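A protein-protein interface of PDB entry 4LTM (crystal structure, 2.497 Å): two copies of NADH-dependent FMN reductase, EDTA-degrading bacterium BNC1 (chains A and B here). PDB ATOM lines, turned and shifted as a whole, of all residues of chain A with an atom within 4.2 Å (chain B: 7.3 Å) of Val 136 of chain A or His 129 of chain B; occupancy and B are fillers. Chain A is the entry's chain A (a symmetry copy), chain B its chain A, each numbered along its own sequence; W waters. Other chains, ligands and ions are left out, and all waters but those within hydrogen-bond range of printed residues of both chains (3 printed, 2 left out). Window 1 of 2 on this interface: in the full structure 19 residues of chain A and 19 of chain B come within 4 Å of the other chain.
A ring nitrogen (NE2) of His 129 of chain A sits at hydrogen-bond distance from the guanidinium group of Arg 125 of chain B (3.0 Å).
NH1 of Arg 125 of chain A is in hydrogen-bond range of NE2 of His 129 of chain B (3.0 Å).
A ring nitrogen (ND1) of His 135 of chain B sits at hydrogen-bond distance from a ring nitrogen (ND1) of His 135 of chain A, 3.4 Å away.
O of Val 136 of chain B lies within hydrogen-bond range of NH1 of Arg 125 of chain B (3.0 Å).
The backbone carbonyl oxygen (O) of His 135 of chain A is in hydrogen-bond range of the backbone NH (N) of Ala 105 of chain A, 2.8 Å away.
OD1 of Asp 121 of chain A lies within salt-bridge range of NE of Arg 125 of chain A, 3.0 Å away.
O of Val 136 of chain A sits at hydrogen-bond distance from NH1 of Arg 125 of chain A, at 3.0 Å.
NH2 of Arg 125 of chain A sits at hydrogen-bond distance from O of Val 137 of chain A (2.9 Å).
Among the printed residues, pairs that only touch across the chains: Asp 121 of chain A with Pro 126 of chain B (3.6 Å), Asp 121 of chain A with His 129 of chain B (3.9 Å), His 129 of chain A with Val 136 of chain B (3.8 Å), His 135 of chain A with Arg 134 of chain B (3.0 Å) and Val 136 of chain A with His 129 of chain B (3.8 Å).
Pro 107 of chain A touches none of the printed residues of chain B.
Printed residues of chain B within 4 Å of Arg 125 of chain A: His 129 (3.0 Å).
Of chain B, only His 129 comes within 4 Å of Val 136 of chain A.
Printed residues of chain A within 4 Å of Arg 134 of chain B: His 135 (3.0 Å).
Of the printed residues of chain A, Val 136 of chain B touches His 129.
The nearest residue of chain B that does not touch Val 136 of chain A is Arg 134 of chain B (5.1 Å).
Hydrophobic or aromatic side chains of chain A that line the printed part of chain B: His 129 and His 135.
Along chain A the printed residues that touch a printed residue of chain B span positions 121 to 136.
Hydrophobic or aromatic side chains of chain B that line the printed part of chain A: Pro 126, His 129 and His 135.
Arg 125 of chain A touches His 129 of chain B, and with the chains exchanged His 129 of chain A touches Arg 125 of chain B.
His 129 of chain A touches Val 136 of chain B, and with the chains exchanged Val 136 of chain A touches His 129 of chain B.
His 135 of chain B touches its own counterpart, His 135 of chain A.
Positions printed for both chains: 125, 129, 133, 135 and 136.
Of the 8 pairs that touch across the chains among the printed residues, 5 have their exchanged pair printed and touching as well.
Water W1 bridges OD2 of Asp 121 of chain A (2.4 Å) and O of Pro 126 of chain B (2.9 Å).
Water W3 lies within hydrogen-bond range of N of Val 136 of chain A (2.8 Å), O of Val 136 of chain B (3.0 Å) and NE2 of His 129 of chain A (3.4 Å).
Water W2 lies within hydrogen-bond range of the backbone NH (N) of Val 136 of chain B (2.8 Å), the backbone carbonyl oxygen (O) of Val 136 of chain A (3.0 Å) and a ring nitrogen (NE2) of His 129 of chain B (3.4 Å).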
ATOM      1  N   ALA A 105     -20.608   4.823   0.027  1.00  0.00           N
ATOM      2  CA  ALA A 105     -20.964   6.189   0.423  1.00  0.00           C
ATOM      3  C   ALA A 105     -19.968   7.222  -0.067  1.00  0.00           C
ATOM      4  O   ALA A 105     -18.772   6.954  -0.136  1.00  0.00           O
ATOM      5  CB  ALA A 105     -21.122   6.301   1.938  1.00  0.00           C
ATOM      6  N   PRO A 107     -18.936  11.121   0.859  1.00  0.00           N
ATOM      7  CA  PRO A 107     -19.096  12.297   1.721  1.00  0.00           C
ATOM      8  C   PRO A 107     -18.740  13.600   0.999  1.00  0.00           C
ATOM      9  O   PRO A 107     -17.646  13.731   0.430  1.00  0.00           O
ATOM     10  CB  PRO A 107     -18.122  12.030   2.889  1.00  0.00           C
ATOM     11  CG  PRO A 107     -17.436  10.727   2.581  1.00  0.00           C
ATOM     12  CD  PRO A 107     -17.668  10.426   1.116  1.00  0.00           C
ATOM     13  N   ASP A 121     -13.369  13.797   7.137  1.00  0.00           N
ATOM     14  CA  ASP A 121     -12.606  12.604   7.502  1.00  0.00           C
ATOM     15  C   ASP A 121     -12.555  12.348   9.008  1.00  0.00           C
ATOM     16  O   ASP A 121     -12.555  11.201   9.442  1.00  0.00           O
ATOM     17  CB  ASP A 121     -11.185  12.653   6.922  1.00  0.00           C
ATOM     18  CG  ASP A 121     -11.145  12.361   5.416  1.00  0.00           C
ATOM     19  OD1 ASP A 121     -12.181  11.944   4.849  1.00  0.00           O
ATOM     20  OD2 ASP A 121     -10.066  12.529   4.805  1.00  0.00           O
ATOM     21  N   ARG A 125     -16.885  10.612   8.699  1.00  0.00           N
ATOM     22  CA  ARG A 125     -16.448   9.263   8.351  1.00  0.00           C
ATOM     23  C   ARG A 125     -16.591   8.242   9.503  1.00  0.00           C
ATOM     24  O   ARG A 125     -17.121   7.148   9.294  1.00  0.00           O
ATOM     25  CB  ARG A 125     -15.028   9.303   7.764  1.00  0.00           C
ATOM     26  CG  ARG A 125     -14.589   8.050   7.048  1.00  0.00           C
ATOM     27  CD  ARG A 125     -13.209   8.233   6.422  1.00  0.00           C
ATOM     28  NE  ARG A 125     -13.237   9.134   5.277  1.00  0.00           N
ATOM     29  CZ  ARG A 125     -13.419   8.742   4.020  1.00  0.00           C
ATOM     30  NH1 ARG A 125     -13.589   7.459   3.740  1.00  0.00           N
ATOM     31  NH2 ARG A 125     -13.442   9.635   3.036  1.00  0.00           N
ATOM     32  N   HIS A 129     -19.034   4.763   9.647  1.00  0.00           N
ATOM     33  CA  HIS A 129     -18.446   3.479  10.029  1.00  0.00           C
ATOM     34  C   HIS A 129     -19.044   2.816  11.274  1.00  0.00           C
ATOM     35  O   HIS A 129     -18.957   1.599  11.420  1.00  0.00           O
ATOM     36  CB  HIS A 129     -16.923   3.569  10.109  1.00  0.00           C
ATOM     37  CG  HIS A 129     -16.272   3.378   8.781  1.00  0.00           C
ATOM     38  ND1 HIS A 129     -16.159   2.138   8.190  1.00  0.00           N
ATOM     39  CD2 HIS A 129     -15.785   4.269   7.888  1.00  0.00           C
ATOM     40  CE1 HIS A 129     -15.596   2.271   7.001  1.00  0.00           C
ATOM     41  NE2 HIS A 129     -15.365   3.554   6.792  1.00  0.00           N
ATOM     42  N   VAL A 133     -21.118   0.672   7.394  1.00  0.00           N
ATOM     43  CA  VAL A 133     -20.967   1.002   5.975  1.00  0.00           C
ATOM     44  C   VAL A 133     -19.946   0.082   5.272  1.00  0.00           C
ATOM     45  O   VAL A 133     -18.985  -0.369   5.885  1.00  0.00           O
ATOM     46  CB  VAL A 133     -20.561   2.484   5.814  1.00  0.00           C
ATOM     47  CG1 VAL A 133     -19.101   2.679   6.240  1.00  0.00           C
ATOM     48  CG2 VAL A 133     -20.813   2.979   4.383  1.00  0.00           C
ATOM     49  N   HIS A 135     -18.233   0.726   2.119  1.00  0.00           N
ATOM     50  CA  HIS A 135     -17.151   1.367   1.382  1.00  0.00           C
ATOM     51  C   HIS A 135     -17.425   2.859   1.286  1.00  0.00           C
ATOM     52  O   HIS A 135     -18.333   3.285   0.561  1.00  0.00           O
ATOM     53  CB  HIS A 135     -17.034   0.746  -0.024  1.00  0.00           C
ATOM     54  CG  HIS A 135     -15.799   1.144  -0.780  1.00  0.00           C
ATOM     55  ND1 HIS A 135     -14.925   2.117  -0.339  1.00  0.00           N
ATOM     56  CD2 HIS A 135     -15.291   0.687  -1.948  1.00  0.00           C
ATOM     57  CE1 HIS A 135     -13.938   2.251  -1.209  1.00  0.00           C
ATOM     58  NE2 HIS A 135     -14.131   1.386  -2.188  1.00  0.00           N
ATOM     59  N   VAL A 136     -16.650   3.649   2.026  1.00  0.00           N
ATOM     60  CA  VAL A 136     -16.729   5.107   1.944  1.00  0.00           C
ATOM     61  C   VAL A 136     -15.533   5.613   1.152  1.00  0.00           C
ATOM     62  O   VAL A 136     -14.401   5.505   1.614  1.00  0.00           O
ATOM     63  CB  VAL A 136     -16.666   5.751   3.339  1.00  0.00           C
ATOM     64  CG1 VAL A 136     -16.942   7.247   3.252  1.00  0.00           C
ATOM     65  CG2 VAL A 136     -17.641   5.082   4.271  1.00  0.00           C
ATOM     66  N   VAL A 137     -15.772   6.170  -0.033  1.00  0.00           N
ATOM     67  CA  VAL A 137     -14.671   6.627  -0.882  1.00  0.00           C
ATOM     68  C   VAL A 137     -14.138   7.963  -0.357  1.00  0.00           C
ATOM     69  O   VAL A 137     -14.555   8.422   0.705  1.00  0.00           O
ATOM     70  CB  VAL A 137     -15.102   6.730  -2.371  1.00  0.00           C
ATOM     71  CG1 VAL A 137     -15.636   5.389  -2.874  1.00  0.00           C
ATOM     72  CG2 VAL A 137     -16.160   7.806  -2.551  1.00  0.00           C
ATOM     73  N   GLN B  97       3.530  10.753  -0.983  1.00  0.00           N
ATOM     74  CA  GLN B  97       2.319  11.477  -0.612  1.00  0.00           C
ATOM     75  C   GLN B  97       1.007  10.721  -0.813  1.00  0.00           C
ATOM     76  O   GLN B  97       0.125  10.757   0.053  1.00  0.00           O
ATOM     77  CB  GLN B  97       2.245  12.826  -1.324  1.00  0.00           C
ATOM     78  CG  GLN B  97       1.055  13.663  -0.869  1.00  0.00           C
ATOM     79  CD  GLN B  97       1.041  15.049  -1.484  1.00  0.00           C
ATOM     80  OE1 GLN B  97       2.024  15.481  -2.081  1.00  0.00           O
ATOM     81  NE2 GLN B  97      -0.079  15.754  -1.337  1.00  0.00           N
ATOM     82  N   PHE B  98       0.866  10.057  -1.953  1.00  0.00           N
ATOM     83  CA  PHE B  98      -0.353   9.302  -2.213  1.00  0.00           C
ATOM     84  C   PHE B  98      -0.025   7.826  -2.346  1.00  0.00           C
ATOM     85  O   PHE B  98      -0.488   7.153  -3.265  1.00  0.00           O
ATOM     86  CB  PHE B  98      -1.070   9.835  -3.452  1.00  0.00           C
ATOM     87  CG  PHE B  98      -1.570  11.240  -3.287  1.00  0.00           C
ATOM     88  CD1 PHE B  98      -2.648  11.509  -2.452  1.00  0.00           C
ATOM     89  CD2 PHE B  98      -0.959  12.294  -3.945  1.00  0.00           C
ATOM     90  CE1 PHE B  98      -3.115  12.811  -2.285  1.00  0.00           C
ATOM     91  CE2 PHE B  98      -1.416  13.595  -3.783  1.00  0.00           C
ATOM     92  CZ  PHE B  98      -2.499  13.854  -2.949  1.00  0.00           C
ATOM     93  N   LEU B 100      -0.909   5.180  -0.934  1.00  0.00           N
ATOM     94  CA  LEU B 100      -1.888   4.123  -0.758  1.00  0.00           C
ATOM     95  C   LEU B 100      -2.923   4.094  -1.883  1.00  0.00           C
ATOM     96  O   LEU B 100      -3.876   3.323  -1.835  1.00  0.00           O
ATOM     97  CB  LEU B 100      -2.557   4.224   0.614  1.00  0.00           C
ATOM     98  CG  LEU B 100      -1.600   4.231   1.814  1.00  0.00           C
ATOM     99  CD1 LEU B 100      -2.337   3.964   3.133  1.00  0.00           C
ATOM    100  CD2 LEU B 100      -0.475   3.241   1.621  1.00  0.00           C
ATOM    101  N   LEU B 124      -6.491   6.773  13.122  1.00  0.00           N
ATOM    102  CA  LEU B 124      -5.736   6.136  12.052  1.00  0.00           C
ATOM    103  C   LEU B 124      -6.394   6.275  10.673  1.00  0.00           C
ATOM    104  O   LEU B 124      -5.727   6.546   9.665  1.00  0.00           O
ATOM    105  CB  LEU B 124      -5.502   4.661  12.386  1.00  0.00           C
ATOM    106  CG  LEU B 124      -4.652   3.902  11.364  1.00  0.00           C
ATOM    107  CD1 LEU B 124      -3.303   4.611  11.137  1.00  0.00           C
ATOM    108  CD2 LEU B 124      -4.456   2.464  11.813  1.00  0.00           C
ATOM    109  N   ARG B 125      -7.706   6.085  10.632  1.00  0.00           N
ATOM    110  CA  ARG B 125      -8.448   6.131   9.376  1.00  0.00           C
ATOM    111  C   ARG B 125      -8.238   7.436   8.573  1.00  0.00           C
ATOM    112  O   ARG B 125      -7.976   7.383   7.368  1.00  0.00           O
ATOM    113  CB  ARG B 125      -9.932   5.817   9.626  1.00  0.00           C
ATOM    114  CG  ARG B 125     -10.740   5.490   8.396  1.00  0.00           C
ATOM    115  CD  ARG B 125     -12.168   5.101   8.767  1.00  0.00           C
ATOM    116  NE  ARG B 125     -12.234   3.799   9.418  1.00  0.00           N
ATOM    117  CZ  ARG B 125     -12.412   2.649   8.775  1.00  0.00           C
ATOM    118  NH1 ARG B 125     -12.546   2.635   7.458  1.00  0.00           N
ATOM    119  NH2 ARG B 125     -12.448   1.504   9.448  1.00  0.00           N
ATOM    120  N   PRO B 126      -8.319   8.609   9.230  1.00  0.00           N
ATOM    121  CA  PRO B 126      -8.027   9.833   8.461  1.00  0.00           C
ATOM    122  C   PRO B 126      -6.590   9.909   7.915  1.00  0.00           C
ATOM    123  O   PRO B 126      -6.377  10.481   6.841  1.00  0.00           O
ATOM    124  CB  PRO B 126      -8.261  10.953   9.479  1.00  0.00           C
ATOM    125  CG  PRO B 126      -9.224  10.373  10.457  1.00  0.00           C
ATOM    126  CD  PRO B 126      -8.837   8.918  10.574  1.00  0.00           C
ATOM    127  N   VAL B 127      -5.619   9.357   8.638  1.00  0.00           N
ATOM    128  CA  VAL B 127      -4.248   9.342   8.143  1.00  0.00           C
ATOM    129  C   VAL B 127      -4.145   8.549   6.841  1.00  0.00           C
ATOM    130  O   VAL B 127      -3.593   9.040   5.864  1.00  0.00           O
ATOM    131  CB  VAL B 127      -3.255   8.795   9.194  1.00  0.00           C
ATOM    132  CG1 VAL B 127      -1.886   8.512   8.559  1.00  0.00           C
ATOM    133  CG2 VAL B 127      -3.139   9.764  10.379  1.00  0.00           C
ATOM    134  N   LEU B 128      -4.699   7.339   6.814  1.00  0.00           N
ATOM    135  CA  LEU B 128      -4.687   6.528   5.589  1.00  0.00           C
ATOM    136  C   LEU B 128      -5.389   7.232   4.430  1.00  0.00           C
ATOM    137  O   LEU B 128      -4.923   7.177   3.294  1.00  0.00           O
ATOM    138  CB  LEU B 128      -5.324   5.155   5.822  1.00  0.00           C
ATOM    139  CG  LEU B 128      -4.759   4.353   6.995  1.00  0.00           C
ATOM    140  CD1 LEU B 128      -5.578   3.088   7.243  1.00  0.00           C
ATOM    141  CD2 LEU B 128      -3.272   4.031   6.778  1.00  0.00           C
ATOM    142  N   HIS B 129      -6.500   7.903   4.720  1.00  0.00           N
ATOM    143  CA  HIS B 129      -7.210   8.662   3.690  1.00  0.00           C
ATOM    144  C   HIS B 129      -6.480   9.893   3.145  1.00  0.00           C
ATOM    145  O   HIS B 129      -6.751  10.319   2.025  1.00  0.00           O
ATOM    146  CB  HIS B 129      -8.634   8.995   4.131  1.00  0.00           C
ATOM    147  CG  HIS B 129      -9.589   7.884   3.855  1.00  0.00           C
ATOM    148  ND1 HIS B 129     -10.055   7.614   2.586  1.00  0.00           N
ATOM    149  CD2 HIS B 129     -10.094   6.919   4.658  1.00  0.00           C
ATOM    150  CE1 HIS B 129     -10.836   6.548   2.626  1.00  0.00           C
ATOM    151  NE2 HIS B 129     -10.871   6.104   3.869  1.00  0.00           N
ATOM    152  N   SER B 130      -5.502  10.409   3.842  1.00  0.00           N
ATOM    153  CA  SER B 130      -4.674  11.429   3.307  1.00  0.00           C
ATOM    154  C   SER B 130      -3.608  10.893   2.378  1.00  0.00           C
ATOM    155  O   SER B 130      -3.036  11.619   1.638  1.00  0.00           O
ATOM    156  CB  SER B 130      -4.075  12.258   4.428  1.00  0.00           C
ATOM    157  OG  SER B 130      -2.833  11.806   4.811  1.00  0.00           O
ATOM    158  N   MET B 131      -3.376   9.601   2.417  1.00  0.00           N
ATOM    159  CA  MET B 131      -2.456   8.983   1.538  1.00  0.00           C
ATOM    160  C   MET B 131      -3.133   8.402   0.332  1.00  0.00           C
ATOM    161  O   MET B 131      -2.533   7.618  -0.320  1.00  0.00           O
ATOM    162  CB  MET B 131      -1.615   7.974   2.265  1.00  0.00           C
ATOM    163  CG  MET B 131      -0.973   8.582   3.483  1.00  0.00           C
ATOM    164  SD  MET B 131       0.089   7.258   4.432  1.00  0.00           S
ATOM    165  CE  MET B 131       1.459   7.376   3.117  1.00  0.00           C
ATOM    166  N   GLY B 132      -4.375   8.761   0.068  1.00  0.00           N
ATOM    167  CA  GLY B 132      -5.117   8.341  -1.107  1.00  0.00           C
ATOM    168  C   GLY B 132      -5.612   6.915  -1.212  1.00  0.00           C
ATOM    169  O   GLY B 132      -5.844   6.419  -2.268  1.00  0.00           O
ATOM    170  N   VAL B 133      -5.751   6.277  -0.072  1.00  0.00           N
ATOM    171  CA  VAL B 133      -6.154   4.871   0.023  1.00  0.00           C
ATOM    172  C   VAL B 133      -7.456   4.588  -0.756  1.00  0.00           C
ATOM    173  O   VAL B 133      -8.321   5.450  -0.862  1.00  0.00           O
ATOM    174  CB  VAL B 133      -6.310   4.461   1.504  1.00  0.00           C
ATOM    175  CG1 VAL B 133      -7.576   5.091   2.095  1.00  0.00           C
ATOM    176  CG2 VAL B 133      -6.299   2.934   1.665  1.00  0.00           C
ATOM    177  N   ARG B 134      -7.580   3.394  -1.328  1.00  0.00           N
ATOM    178  CA  ARG B 134      -8.758   3.074  -2.128  1.00  0.00           C
ATOM    179  C   ARG B 134      -9.940   2.639  -1.265  1.00  0.00           C
ATOM    180  O   ARG B 134     -11.064   3.116  -1.445  1.00  0.00           O
ATOM    181  CB  ARG B 134      -8.445   1.995  -3.173  1.00  0.00           C
ATOM    182  CG  ARG B 134      -9.574   1.754  -4.174  1.00  0.00           C
ATOM    183  CD  ARG B 134      -9.163   0.765  -5.272  1.00  0.00           C
ATOM    184  NE  ARG B 134      -8.743  -0.513  -4.706  1.00  0.00           N
ATOM    185  CZ  ARG B 134      -9.590  -1.417  -4.220  1.00  0.00           C
ATOM    186  NH1 ARG B 134      -9.131  -2.548  -3.711  1.00  0.00           N
ATOM    187  NH2 ARG B 134     -10.902  -1.183  -4.242  1.00  0.00           N
ATOM    188  N   HIS B 135      -9.685   1.736  -0.323  1.00  0.00           N
ATOM    189  CA  HIS B 135     -10.770   1.085   0.401  1.00  0.00           C
ATOM    190  C   HIS B 135     -10.259   0.610   1.751  1.00  0.00           C
ATOM    191  O   HIS B 135      -9.473  -0.344   1.826  1.00  0.00           O
ATOM    192  CB  HIS B 135     -11.309  -0.104  -0.421  1.00  0.00           C
ATOM    193  CG  HIS B 135     -12.589  -0.691   0.100  1.00  0.00           C
ATOM    194  ND1 HIS B 135     -13.151  -0.326   1.308  1.00  0.00           N
ATOM    195  CD2 HIS B 135     -13.421  -1.616  -0.433  1.00  0.00           C
ATOM    196  CE1 HIS B 135     -14.266  -1.010   1.500  1.00  0.00           C
ATOM    197  NE2 HIS B 135     -14.458  -1.791   0.453  1.00  0.00           N
ATOM    198  N   VAL B 136     -10.690   1.284   2.814  1.00  0.00           N
ATOM    199  CA  VAL B 136     -10.369   0.867   4.179  1.00  0.00           C
ATOM    200  C   VAL B 136     -11.599   0.213   4.788  1.00  0.00           C
ATOM    201  O   VAL B 136     -12.599   0.885   5.022  1.00  0.00           O
ATOM    202  CB  VAL B 136     -10.000   2.072   5.060  1.00  0.00           C
ATOM    203  CG1 VAL B 136      -9.483   1.605   6.417  1.00  0.00           C
ATOM    204  CG2 VAL B 136      -8.979   2.936   4.369  1.00  0.00           C
ATOM    205  N   GLY B 185      -8.767   6.396  -5.455  1.00  0.00           N
ATOM    206  CA  GLY B 185      -8.460   6.929  -4.141  1.00  0.00           C
ATOM    207  C   GLY B 185      -7.635   8.194  -4.258  1.00  0.00           C
ATOM    208  O   GLY B 185      -7.736   9.100  -3.431  1.00  0.00           O
ATOM    209  N   PRO B 187      -6.770  11.779  -5.615  1.00  0.00           N
ATOM    210  CA  PRO B 187      -7.602  12.909  -6.059  1.00  0.00           C
ATOM    211  C   PRO B 187      -7.404  13.302  -7.532  1.00  0.00           C
ATOM    212  O   PRO B 187      -8.324  13.860  -8.131  1.00  0.00           O
ATOM    213  CB  PRO B 187      -7.165  14.059  -5.134  1.00  0.00           C
ATOM    214  CG  PRO B 187      -5.837  13.645  -4.594  1.00  0.00           C
ATOM    215  CD  PRO B 187      -5.883  12.149  -4.499  1.00  0.00           C
HETATM  216  O   HOH W   1      -7.752  12.712   5.499  1.00  0.00           O
HETATM  217  O   HOH W   2     -12.355   3.492   2.381  1.00  0.00           O
HETATM  218  O   HOH W   3     -14.753   2.440   3.690  1.00  0.00           O
